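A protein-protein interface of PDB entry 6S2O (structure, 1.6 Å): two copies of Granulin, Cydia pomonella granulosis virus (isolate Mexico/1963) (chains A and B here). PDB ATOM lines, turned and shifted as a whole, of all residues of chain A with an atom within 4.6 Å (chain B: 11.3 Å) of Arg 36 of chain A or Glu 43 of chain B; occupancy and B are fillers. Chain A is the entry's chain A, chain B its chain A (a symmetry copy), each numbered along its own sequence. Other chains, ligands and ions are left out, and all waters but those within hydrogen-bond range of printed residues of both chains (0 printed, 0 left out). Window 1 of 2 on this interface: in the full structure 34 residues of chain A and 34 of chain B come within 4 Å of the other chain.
The guanidinium group (NH2) of Arg 35 of chain A lies close to the side-chain carboxylate (OE2) of Glu 43 of chain B (2.8 Å).
Of the 11 printed residues of chain A, 4 touch a printed residue of chain B. Hydrophobic or aromatic side chains of chain A within 4 Å of the printed part of chain B: Leu 7. Among the printed residues, 6 pairs touch across the chains.
9 positions are printed for both chains. Of the 6 pairs that touch across the chains among the printed residues, none has its exchanged pair printed and touching as well.
Of the printed residues of chain B, Leu 7 of chain A touches Glu 43, Ala 44 and Glu 47. Asn 32 of chain A touches just one residue of chain B: Ile 50 (3.7 Å). No residue of chain B comes within 4 Å of Asp 33 of chain A. No residue of chain B comes within 4 Å of Val 34 of chain A. Arg 36 of chain A touches one residue of chain B. Asp 39 of chain A touches none of the printed residues of chain B. No residue of chain B comes within 4 Å of Arg 40 of chain A. Glu 43 of chain B touches just these residues of chain A: Leu 7, Arg 35 and Arg 36. Printed residues of chain A within 4 Å of Ala 44 of chain B: Leu 7 (3.5 Å). Glu 45 of chain B touches none of the printed residues of chain A. Printed residues of chain A within 4 Å of Glu 47 of chain B: Leu 7 (3.5 Å). Of the printed residues of chain A, Ile 50 of chain B touches Asn 32 (3.7 Å). The nearest residue of chain B that does not touch Arg 36 of chain A is Ile 50 of chain B (7.3 Å). The nearest printed residue of chain A that does not touch Ala 44 of chain B is Arg 35 of chain A (7.8 Å).
Among the printed residues, merely in contact across the chains: Leu 7 of chain A with Ala 44 of chain B, Leu 7 of chain A with Glu 47 of chain B, Leu 7 of chain A with Glu 43 of chain B, Asn 32 of chain A with Ile 50 of chain B and Arg 36 of chain A with Glu 43 of chain B.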
ATOM      1  N   LEU A   7       3.109  13.994  13.236  1.00  0.00           N
ATOM      2  CA  LEU A   7       4.413  14.618  13.013  1.00  0.00           C
ATOM      3  C   LEU A   7       5.044  15.041  14.332  1.00  0.00           C
ATOM      4  O   LEU A   7       4.431  15.766  15.119  1.00  0.00           O
ATOM      5  CB  LEU A   7       4.262  15.836  12.099  1.00  0.00           C
ATOM      6  CG  LEU A   7       3.954  15.585  10.626  1.00  0.00           C
ATOM      7  CD1 LEU A   7       3.668  16.898   9.914  1.00  0.00           C
ATOM      8  CD2 LEU A   7       5.117  14.877   9.977  1.00  0.00           C
ATOM      9  N   ARG A  11       6.731  21.117  11.500  1.00  0.00           N
ATOM     10  CA  ARG A  11       7.452  21.271  10.244  1.00  0.00           C
ATOM     11  C   ARG A  11       8.745  22.035  10.495  1.00  0.00           C
ATOM     12  O   ARG A  11       9.188  22.830   9.664  1.00  0.00           O
ATOM     13  CB  ARG A  11       6.598  21.972   9.187  1.00  0.00           C
ATOM     14  CG  ARG A  11       5.431  21.158   8.624  1.00  0.00           C
ATOM     15  CD  ARG A  11       4.281  21.078   9.619  1.00  0.00           C
ATOM     16  NE  ARG A  11       2.982  21.386   9.032  1.00  0.00           N
ATOM     17  CZ  ARG A  11       1.840  21.233   9.691  1.00  0.00           C
ATOM     18  NH1 ARG A  11       1.873  20.744  10.916  1.00  0.00           N
ATOM     19  NH2 ARG A  11       0.676  21.535   9.129  1.00  0.00           N
ATOM     20  N   ASN A  32      12.939  19.239   1.413  1.00  0.00           N
ATOM     21  CA  ASN A  32      11.532  19.505   1.705  1.00  0.00           C
ATOM     22  C   ASN A  32      11.068  20.788   1.039  1.00  0.00           C
ATOM     23  O   ASN A  32       9.931  20.870   0.563  1.00  0.00           O
ATOM     24  CB  ASN A  32      11.313  19.619   3.211  1.00  0.00           C
ATOM     25  CG  ASN A  32      10.863  18.339   3.824  1.00  0.00           C
ATOM     26  OD1 ASN A  32      10.571  17.367   3.122  1.00  0.00           O
ATOM     27  ND2 ASN A  32      10.797  18.316   5.151  1.00  0.00           N
ATOM     28  N   ASP A  33      11.928  21.810   1.029  1.00  0.00           N
ATOM     29  CA  ASP A  33      11.586  23.067   0.367  1.00  0.00           C
ATOM     30  C   ASP A  33      11.378  22.864  -1.126  1.00  0.00           C
ATOM     31  O   ASP A  33      10.478  23.465  -1.719  1.00  0.00           O
ATOM     32  CB  ASP A  33      12.676  24.112   0.610  1.00  0.00           C
ATOM     33  CG  ASP A  33      12.596  24.741   2.010  1.00  0.00           C
ATOM     34  OD1 ASP A  33      11.680  24.384   2.787  1.00  0.00           O
ATOM     35  OD2 ASP A  33      13.452  25.593   2.336  1.00  0.00           O
ATOM     36  N   VAL A  34      12.210  22.036  -1.754  1.00  0.00           N
ATOM     37  CA  VAL A  34      12.031  21.712  -3.163  1.00  0.00           C
ATOM     38  C   VAL A  34      10.751  20.909  -3.382  1.00  0.00           C
ATOM     39  O   VAL A  34      10.003  21.156  -4.336  1.00  0.00           O
ATOM     40  CB  VAL A  34      13.268  20.958  -3.683  1.00  0.00           C
ATOM     41  CG1 VAL A  34      13.035  20.487  -5.106  1.00  0.00           C
ATOM     42  CG2 VAL A  34      14.519  21.836  -3.584  1.00  0.00           C
ATOM     43  N   ARG A  35      10.474  19.934  -2.513  1.00  0.00           N
ATOM     44  CA  ARG A  35       9.239  19.162  -2.659  1.00  0.00           C
ATOM     45  C   ARG A  35       8.010  20.035  -2.411  1.00  0.00           C
ATOM     46  O   ARG A  35       6.976  19.859  -3.065  1.00  0.00           O
ATOM     47  CB  ARG A  35       9.240  17.959  -1.711  1.00  0.00           C
ATOM     48  CG  ARG A  35       8.012  17.050  -1.871  1.00  0.00           C
ATOM     49  CD  ARG A  35       8.071  15.845  -0.952  1.00  0.00           C
ATOM     50  NE  ARG A  35       8.368  16.243   0.417  1.00  0.00           N
ATOM     51  CZ  ARG A  35       7.487  16.801   1.243  1.00  0.00           C
ATOM     52  NH1 ARG A  35       6.237  17.022   0.849  1.00  0.00           N
ATOM     53  NH2 ARG A  35       7.859  17.138   2.469  1.00  0.00           N
ATOM     54  N   ARG A  36       8.107  20.988  -1.488  1.00  0.00           N
ATOM     55  CA  ARG A  36       6.967  21.852  -1.211  1.00  0.00           C
ATOM     56  C   ARG A  36       6.709  22.839  -2.347  1.00  0.00           C
ATOM     57  O   ARG A  36       5.548  23.182  -2.609  1.00  0.00           O
ATOM     58  CB  ARG A  36       7.175  22.580   0.116  1.00  0.00           C
ATOM     59  CG  ARG A  36       6.891  21.677   1.312  1.00  0.00           C
ATOM     60  CD  ARG A  36       7.451  22.226   2.602  1.00  0.00           C
ATOM     61  NE  ARG A  36       7.266  21.272   3.696  1.00  0.00           N
ATOM     62  CZ  ARG A  36       8.024  21.233   4.787  1.00  0.00           C
ATOM     63  NH1 ARG A  36       9.023  22.094   4.930  1.00  0.00           N
ATOM     64  NH2 ARG A  36       7.785  20.336   5.738  1.00  0.00           N
ATOM     65  N   LYS A  37       7.765  23.289  -3.041  1.00  0.00           N
ATOM     66  CA  LYS A  37       7.577  24.114  -4.235  1.00  0.00           C
ATOM     67  C   LYS A  37       6.842  23.342  -5.326  1.00  0.00           C
ATOM     68  O   LYS A  37       5.962  23.891  -6.001  1.00  0.00           O
ATOM     69  CB  LYS A  37       8.933  24.609  -4.768  1.00  0.00           C
ATOM     70  CG  LYS A  37       8.842  25.470  -6.059  1.00  0.00           C
ATOM     71  CD  LYS A  37       8.241  26.824  -5.725  1.00  0.00           C
ATOM     72  CE  LYS A  37       8.468  27.814  -6.843  1.00  0.00           C
ATOM     73  NZ  LYS A  37       7.882  29.136  -6.478  1.00  0.00           N
ATOM     74  N   LYS A  38       7.249  22.085  -5.557  1.00  0.00           N
ATOM     75  CA  LYS A  38       6.578  21.126  -6.425  1.00  0.00           C
ATOM     76  C   LYS A  38       5.106  21.012  -6.110  1.00  0.00           C
ATOM     77  O   LYS A  38       4.261  21.281  -6.974  1.00  0.00           O
ATOM     78  CB  LYS A  38       7.205  19.749  -6.298  1.00  0.00           C
ATOM     79  CG  LYS A  38       8.128  19.425  -7.372  1.00  0.00           C
ATOM     80  CD  LYS A  38       8.474  17.987  -7.088  1.00  0.00           C
ATOM     81  CE  LYS A  38       7.581  17.115  -7.903  1.00  0.00           C
ATOM     82  NZ  LYS A  38       6.149  17.216  -7.767  1.00  0.00           N
ATOM     83  N   ASP A  39       4.814  20.584  -4.880  1.00  0.00           N
ATOM     84  CA  ASP A  39       3.440  20.386  -4.437  1.00  0.00           C
ATOM     85  C   ASP A  39       2.546  21.585  -4.741  1.00  0.00           C
ATOM     86  O   ASP A  39       1.354  21.415  -5.021  1.00  0.00           O
ATOM     87  CB  ASP A  39       3.424  20.109  -2.930  1.00  0.00           C
ATOM     88  CG  ASP A  39       3.687  18.650  -2.598  1.00  0.00           C
ATOM     89  OD1 ASP A  39       3.869  18.331  -1.399  1.00  0.00           O
ATOM     90  OD2 ASP A  39       3.701  17.826  -3.537  1.00  0.00           O
ATOM     91  N   ARG A  40       3.086  22.799  -4.642  1.00  0.00           N
ATOM     92  CA  ARG A  40       2.330  24.034  -4.821  1.00  0.00           C
ATOM     93  C   ARG A  40       2.215  24.477  -6.256  1.00  0.00           C
ATOM     94  O   ARG A  40       1.230  25.134  -6.608  1.00  0.00           O
ATOM     95  CB  ARG A  40       2.996  25.154  -4.065  1.00  0.00           C
ATOM     96  CG  ARG A  40       2.126  26.246  -3.509  1.00  0.00           C
ATOM     97  CD  ARG A  40       3.172  27.002  -2.887  1.00  0.00           C
ATOM     98  NE  ARG A  40       3.533  26.165  -1.759  1.00  0.00           N
ATOM     99  CZ  ARG A  40       4.778  26.019  -1.331  1.00  0.00           C
ATOM    100  NH1 ARG A  40       5.794  26.570  -2.015  1.00  0.00           N
ATOM    101  NH2 ARG A  40       4.994  25.225  -0.292  1.00  0.00           N
ATOM    102  N   SER B   6       0.875  33.044  -7.997  1.00  0.00           N
ATOM    103  CA  SER B   6       0.187  32.027  -8.787  1.00  0.00           C
ATOM    104  C   SER B   6      -1.265  31.829  -8.323  1.00  0.00           C
ATOM    105  O   SER B   6      -2.192  32.297  -8.994  1.00  0.00           O
ATOM    106  CB  SER B   6       0.952  30.696  -8.742  1.00  0.00           C
ATOM    107  OG  SER B   6       1.325  30.336  -7.422  1.00  0.00           O
ATOM    108  N   LEU B   7      -1.453  31.140  -7.191  1.00  0.00           N
ATOM    109  CA  LEU B   7      -2.786  30.900  -6.639  1.00  0.00           C
ATOM    110  C   LEU B   7      -3.548  32.208  -6.477  1.00  0.00           C
ATOM    111  O   LEU B   7      -3.062  33.144  -5.839  1.00  0.00           O
ATOM    112  CB  LEU B   7      -2.674  30.196  -5.285  1.00  0.00           C
ATOM    113  CG  LEU B   7      -2.236  28.734  -5.278  1.00  0.00           C
ATOM    114  CD1 LEU B   7      -2.013  28.256  -3.852  1.00  0.00           C
ATOM    115  CD2 LEU B   7      -3.281  27.887  -5.961  1.00  0.00           C
ATOM    116  N   ARG B  11      -5.543  30.182  -0.175  1.00  0.00           N
ATOM    117  CA  ARG B  11      -6.179  28.906   0.120  1.00  0.00           C
ATOM    118  C   ARG B  11      -7.549  29.155   0.736  1.00  0.00           C
ATOM    119  O   ARG B  11      -7.995  28.418   1.616  1.00  0.00           O
ATOM    120  CB  ARG B  11      -5.312  28.045   1.040  1.00  0.00           C
ATOM    121  CG  ARG B  11      -4.040  27.471   0.413  1.00  0.00           C
ATOM    122  CD  ARG B  11      -2.964  28.538   0.264  1.00  0.00           C
ATOM    123  NE  ARG B  11      -1.658  28.120   0.757  1.00  0.00           N
ATOM    124  CZ  ARG B  11      -0.559  28.845   0.589  1.00  0.00           C
ATOM    125  NH1 ARG B  11      -0.640  29.976  -0.088  1.00  0.00           N
ATOM    126  NH2 ARG B  11       0.613  28.439   1.061  1.00  0.00           N
ATOM    127  N   VAL B  34     -10.075  16.790   2.398  1.00  0.00           N
ATOM    128  CA  VAL B  34      -9.764  15.369   2.313  1.00  0.00           C
ATOM    129  C   VAL B  34      -8.406  15.145   1.652  1.00  0.00           C
ATOM    130  O   VAL B  34      -7.613  14.307   2.101  1.00  0.00           O
ATOM    131  CB  VAL B  34     -10.888  14.636   1.559  1.00  0.00           C
ATOM    132  CG1 VAL B  34     -10.509  13.184   1.336  1.00  0.00           C
ATOM    133  CG2 VAL B  34     -12.214  14.756   2.315  1.00  0.00           C
ATOM    134  N   ARG B  35      -8.111  15.879   0.576  1.00  0.00           N
ATOM    135  CA  ARG B  35      -6.805  15.727  -0.069  1.00  0.00           C
ATOM    136  C   ARG B  35      -5.679  16.209   0.844  1.00  0.00           C
ATOM    137  O   ARG B  35      -4.588  15.629   0.850  1.00  0.00           O
ATOM    138  CB  ARG B  35      -6.772  16.480  -1.402  1.00  0.00           C
ATOM    139  CG  ARG B  35      -5.461  16.293  -2.181  1.00  0.00           C
ATOM    140  CD  ARG B  35      -5.484  17.011  -3.515  1.00  0.00           C
ATOM    141  NE  ARG B  35      -5.916  18.394  -3.360  1.00  0.00           N
ATOM    142  CZ  ARG B  35      -5.151  19.368  -2.874  1.00  0.00           C
ATOM    143  NH1 ARG B  35      -3.899  19.122  -2.502  1.00  0.00           N
ATOM    144  NH2 ARG B  35      -5.641  20.593  -2.763  1.00  0.00           N
ATOM    145  N   ARG B  36      -5.928  17.253   1.631  1.00  0.00           N
ATOM    146  CA  ARG B  36      -4.892  17.755   2.524  1.00  0.00           C
ATOM    147  C   ARG B  36      -4.636  16.806   3.693  1.00  0.00           C
ATOM    148  O   ARG B  36      -3.494  16.701   4.159  1.00  0.00           O
ATOM    149  CB  ARG B  36      -5.261  19.153   3.016  1.00  0.00           C
ATOM    150  CG  ARG B  36      -4.989  20.220   1.962  1.00  0.00           C
ATOM    151  CD  ARG B  36      -5.690  21.524   2.258  1.00  0.00           C
ATOM    152  NE  ARG B  36      -5.505  22.474   1.161  1.00  0.00           N
ATOM    153  CZ  ARG B  36      -6.336  23.477   0.894  1.00  0.00           C
ATOM    154  NH1 ARG B  36      -7.414  23.659   1.646  1.00  0.00           N
ATOM    155  NH2 ARG B  36      -6.091  24.299  -0.120  1.00  0.00           N
ATOM    156  N   LYS B  37      -5.672  16.099   4.165  1.00  0.00           N
ATOM    157  CA  LYS B  37      -5.469  15.063   5.179  1.00  0.00           C
ATOM    158  C   LYS B  37      -4.590  13.936   4.645  1.00  0.00           C
ATOM    159  O   LYS B  37      -3.713  13.431   5.357  1.00  0.00           O
ATOM    160  CB  LYS B  37      -6.819  14.494   5.648  1.00  0.00           C
ATOM    161  CG  LYS B  37      -6.707  13.359   6.706  1.00  0.00           C
ATOM    162  CD  LYS B  37      -6.254  13.944   8.032  1.00  0.00           C
ATOM    163  CE  LYS B  37      -6.482  12.972   9.165  1.00  0.00           C
ATOM    164  NZ  LYS B  37      -6.042  13.581  10.453  1.00  0.00           N
ATOM    165  N   LYS B  38      -4.867  13.485   3.412  1.00  0.00           N
ATOM    166  CA  LYS B  38      -4.052  12.544   2.654  1.00  0.00           C
ATOM    167  C   LYS B  38      -2.603  12.966   2.602  1.00  0.00           C
ATOM    168  O   LYS B  38      -1.723  12.229   3.066  1.00  0.00           O
ATOM    169  CB  LYS B  38      -4.564  12.408   1.232  1.00  0.00           C
ATOM    170  CG  LYS B  38      -5.373  11.222   1.012  1.00  0.00           C
ATOM    171  CD  LYS B  38      -5.612  11.255  -0.475  1.00  0.00           C
ATOM    172  CE  LYS B  38      -4.588  10.400  -1.139  1.00  0.00           C
ATOM    173  NZ  LYS B  38      -3.185  10.674  -0.954  1.00  0.00           N
ATOM    174  N   ASP B  39      -2.368  14.139   2.010  1.00  0.00           N
ATOM    175  CA  ASP B  39      -1.018  14.665   1.849  1.00  0.00           C
ATOM    176  C   ASP B  39      -0.212  14.624   3.143  1.00  0.00           C
ATOM    177  O   ASP B  39       1.007  14.427   3.109  1.00  0.00           O
ATOM    178  CB  ASP B  39      -1.091  16.109   1.341  1.00  0.00           C
ATOM    179  CG  ASP B  39      -1.250  16.194  -0.168  1.00  0.00           C
ATOM    180  OD1 ASP B  39      -1.493  17.312  -0.683  1.00  0.00           O
ATOM    181  OD2 ASP B  39      -1.122  15.145  -0.833  1.00  0.00           O
ATOM    182  N   ARG B  40      -0.863  14.856   4.284  1.00  0.00           N
ATOM    183  CA  ARG B  40      -0.206  14.931   5.585  1.00  0.00           C
ATOM    184  C   ARG B  40      -0.023  13.595   6.254  1.00  0.00           C
ATOM    185  O   ARG B  40       0.924  13.433   7.030  1.00  0.00           O
ATOM    186  CB  ARG B  40      -1.021  15.786   6.519  1.00  0.00           C
ATOM    187  CG  ARG B  40      -0.294  16.574   7.572  1.00  0.00           C
ATOM    188  CD  ARG B  40      -1.446  17.208   8.141  1.00  0.00           C
ATOM    189  NE  ARG B  40      -1.816  18.162   7.113  1.00  0.00           N
ATOM    190  CZ  ARG B  40      -3.072  18.452   6.809  1.00  0.00           C
ATOM    191  NH1 ARG B  40      -4.078  17.773   7.384  1.00  0.00           N
ATOM    192  NH2 ARG B  40      -3.294  19.338   5.848  1.00  0.00           N
ATOM    193  N   ILE B  41      -0.920  12.644   6.004  1.00  0.00           N
ATOM    194  CA  ILE B  41      -0.586  11.276   6.359  1.00  0.00           C
ATOM    195  C   ILE B  41       0.698  10.885   5.632  1.00  0.00           C
ATOM    196  O   ILE B  41       1.548  10.173   6.185  1.00  0.00           O
ATOM    197  CB  ILE B  41      -1.783  10.360   6.051  1.00  0.00           C
ATOM    198  CG1 ILE B  41      -2.869  10.608   7.112  1.00  0.00           C
ATOM    199  CG2 ILE B  41      -1.362   8.885   5.975  1.00  0.00           C
ATOM    200  CD1 ILE B  41      -4.214   9.980   6.798  1.00  0.00           C
ATOM    201  N   ARG B  42       0.909  11.432   4.432  1.00  0.00           N
ATOM    202  CA  ARG B  42       2.128  11.151   3.671  1.00  0.00           C
ATOM    203  C   ARG B  42       3.346  11.885   4.241  1.00  0.00           C
ATOM    204  O   ARG B  42       4.440  11.313   4.307  1.00  0.00           O
ATOM    205  CB  ARG B  42       1.911  11.513   2.205  1.00  0.00           C
ATOM    206  CG  ARG B  42       2.952  10.954   1.266  1.00  0.00           C
ATOM    207  CD  ARG B  42       3.509  12.044   0.361  1.00  0.00           C
ATOM    208  NE  ARG B  42       2.483  12.673  -0.468  1.00  0.00           N
ATOM    209  CZ  ARG B  42       2.189  13.972  -0.442  1.00  0.00           C
ATOM    210  NH1 ARG B  42       2.841  14.789   0.377  1.00  0.00           N
ATOM    211  NH2 ARG B  42       1.236  14.454  -1.232  1.00  0.00           N
ATOM    212  N   GLU B  43       3.191  13.149   4.652  1.00  0.00           N
ATOM    213  CA  GLU B  43       4.315  13.849   5.272  1.00  0.00           C
ATOM    214  C   GLU B  43       4.726  13.191   6.583  1.00  0.00           C
ATOM    215  O   GLU B  43       5.908  13.204   6.941  1.00  0.00           O
ATOM    216  CB  GLU B  43       3.978  15.322   5.504  1.00  0.00           C
ATOM    217  CG  GLU B  43       4.095  16.166   4.244  1.00  0.00           C
ATOM    218  CD  GLU B  43       5.050  17.339   4.394  1.00  0.00           C
ATOM    219  OE1 GLU B  43       4.620  18.497   4.198  1.00  0.00           O
ATOM    220  OE2 GLU B  43       6.232  17.103   4.710  1.00  0.00           O
ATOM    221  N   ALA B  44       3.775  12.606   7.312  1.00  0.00           N
ATOM    222  CA  ALA B  44       4.136  11.894   8.531  1.00  0.00           C
ATOM    223  C   ALA B  44       4.867  10.595   8.217  1.00  0.00           C
ATOM    224  O   ALA B  44       5.709  10.146   9.006  1.00  0.00           O
ATOM    225  CB  ALA B  44       2.883  11.622   9.377  1.00  0.00           C
ATOM    226  N   GLU B  45       4.575   9.986   7.073  1.00  0.00           N
ATOM    227  CA  GLU B  45       5.302   8.783   6.682  1.00  0.00           C
ATOM    228  C   GLU B  45       6.700   9.093   6.149  1.00  0.00           C
ATOM    229  O   GLU B  45       7.584   8.232   6.215  1.00  0.00           O
ATOM    230  CB  GLU B  45       4.491   7.999   5.646  1.00  0.00           C
ATOM    231  CG  GLU B  45       5.222   6.806   5.041  1.00  0.00           C
ATOM    232  CD  GLU B  45       4.694   6.421   3.671  1.00  0.00           C
ATOM    233  OE1 GLU B  45       4.375   7.329   2.876  1.00  0.00           O
ATOM    234  OE2 GLU B  45       4.597   5.206   3.393  1.00  0.00           O
ATOM    235  N   TYR B  46       6.933  10.304   5.658  1.00  0.00           N
ATOM    236  CA  TYR B  46       8.250  10.656   5.144  1.00  0.00           C
ATOM    237  C   TYR B  46       9.140  11.286   6.194  1.00  0.00           C
ATOM    238  O   TYR B  46      10.341  11.432   5.952  1.00  0.00           O
ATOM    239  CB  TYR B  46       8.134  11.626   3.959  1.00  0.00           C
ATOM    240  CG  TYR B  46       7.501  11.044   2.713  1.00  0.00           C
ATOM    241  CD1 TYR B  46       7.066   9.720   2.677  1.00  0.00           C
ATOM    242  CD2 TYR B  46       7.337  11.822   1.567  1.00  0.00           C
ATOM    243  CE1 TYR B  46       6.479   9.188   1.539  1.00  0.00           C
ATOM    244  CE2 TYR B  46       6.760  11.297   0.421  1.00  0.00           C
ATOM    245  CZ  TYR B  46       6.328   9.980   0.415  1.00  0.00           C
ATOM    246  OH  TYR B  46       5.748   9.452  -0.719  1.00  0.00           O
ATOM    247  N   GLU B  47       8.579  11.690   7.330  1.00  0.00           N
ATOM    248  CA  GLU B  47       9.379  12.382   8.337  1.00  0.00           C
ATOM    249  C   GLU B  47      10.606  11.568   8.745  1.00  0.00           C
ATOM    250  O   GLU B  47      11.708  12.140   8.767  1.00  0.00           O
ATOM    251  CB  GLU B  47       8.496  12.748   9.536  1.00  0.00           C
ATOM    252  CG  GLU B  47       8.845  14.114  10.149  1.00  0.00           C
ATOM    253  CD  GLU B  47       8.214  14.353  11.522  1.00  0.00           C
ATOM    254  OE1 GLU B  47       8.208  15.514  11.983  1.00  0.00           O
ATOM    255  OE2 GLU B  47       7.731  13.382  12.149  1.00  0.00           O
ATOM    256  N   PRO B  48      10.513  10.263   9.048  1.00  0.00           N
ATOM    257  CA  PRO B  48      11.737   9.527   9.439  1.00  0.00           C
ATOM    258  C   PRO B  48      12.795   9.462   8.356  1.00  0.00           C
ATOM    259  O   PRO B  48      13.989   9.347   8.659  1.00  0.00           O
ATOM    260  CB  PRO B  48      11.212   8.119   9.776  1.00  0.00           C
ATOM    261  CG  PRO B  48       9.849   8.047   9.173  1.00  0.00           C
ATOM    262  CD  PRO B  48       9.309   9.428   9.218  1.00  0.00           C
ATOM    263  N   ILE B  49      12.383   9.515   7.097  1.00  0.00           N
ATOM    264  CA  ILE B  49      13.307   9.555   5.975  1.00  0.00           C
ATOM    265  C   ILE B  49      14.044  10.888   5.924  1.00  0.00           C
ATOM    266  O   ILE B  49      15.261  10.931   5.721  1.00  0.00           O
ATOM    267  CB  ILE B  49      12.523   9.295   4.681  1.00  0.00           C
ATOM    268  CG1 ILE B  49      11.842   7.933   4.758  1.00  0.00           C
ATOM    269  CG2 ILE B  49      13.408   9.445   3.506  1.00  0.00           C
ATOM    270  CD1 ILE B  49      10.440   7.955   4.182  1.00  0.00           C
ATOM    271  N   ILE B  50      13.310  11.997   6.076  1.00  0.00           N
ATOM    272  CA  ILE B  50      13.934  13.318   6.111  1.00  0.00           C
ATOM    273  C   ILE B  50      14.925  13.407   7.271  1.00  0.00           C
ATOM    274  O   ILE B  50      15.910  14.152   7.201  1.00  0.00           O
ATOM    275  CB  ILE B  50      12.826  14.399   6.203  1.00  0.00           C
ATOM    276  CG1 ILE B  50      11.990  14.429   4.919  1.00  0.00           C
ATOM    277  CG2 ILE B  50      13.400  15.811   6.524  1.00  0.00           C
ATOM    278  CD1 ILE B  50      12.808  14.451   3.655  1.00  0.00           C
ATOM    279  N   ASP B  51      14.698  12.640   8.352  1.00  0.00           N
ATOM    280  CA  ASP B  51      15.618  12.691   9.491  1.00  0.00           C
ATOM    281  C   ASP B  51      16.972  12.079   9.159  1.00  0.00           C
ATOM    282  O   ASP B  51      17.998  12.526   9.696  1.00  0.00           O
ATOM    283  CB  ASP B  51      15.000  11.986  10.696  1.00  0.00           C
ATOM    284  CG  ASP B  51      15.276  12.709  11.988  1.00  0.00           C
ATOM    285  OD1 ASP B  51      15.819  13.826  11.910  1.00  0.00           O
ATOM    286  OD2 ASP B  51      14.952  12.165  13.076  1.00  0.00           O
ATOM    287  N   ASP B  54      18.681  14.721   7.180  1.00  0.00           N
ATOM    288  CA  ASP B  54      19.104  15.858   8.016  1.00  0.00           C
ATOM    289  C   ASP B  54      20.379  15.591   8.824  1.00  0.00           C
ATOM    290  O   ASP B  54      20.807  16.483   9.573  1.00  0.00           O
ATOM    291  CB  ASP B  54      17.970  16.280   8.965  1.00  0.00           C
ATOM    292  CG  ASP B  54      17.012  17.279   8.323  1.00  0.00           C
ATOM    293  OD1 ASP B  54      17.360  17.785   7.243  1.00  0.00           O
ATOM    294  OD2 ASP B  54      15.909  17.554   8.874  1.00  0.00           O
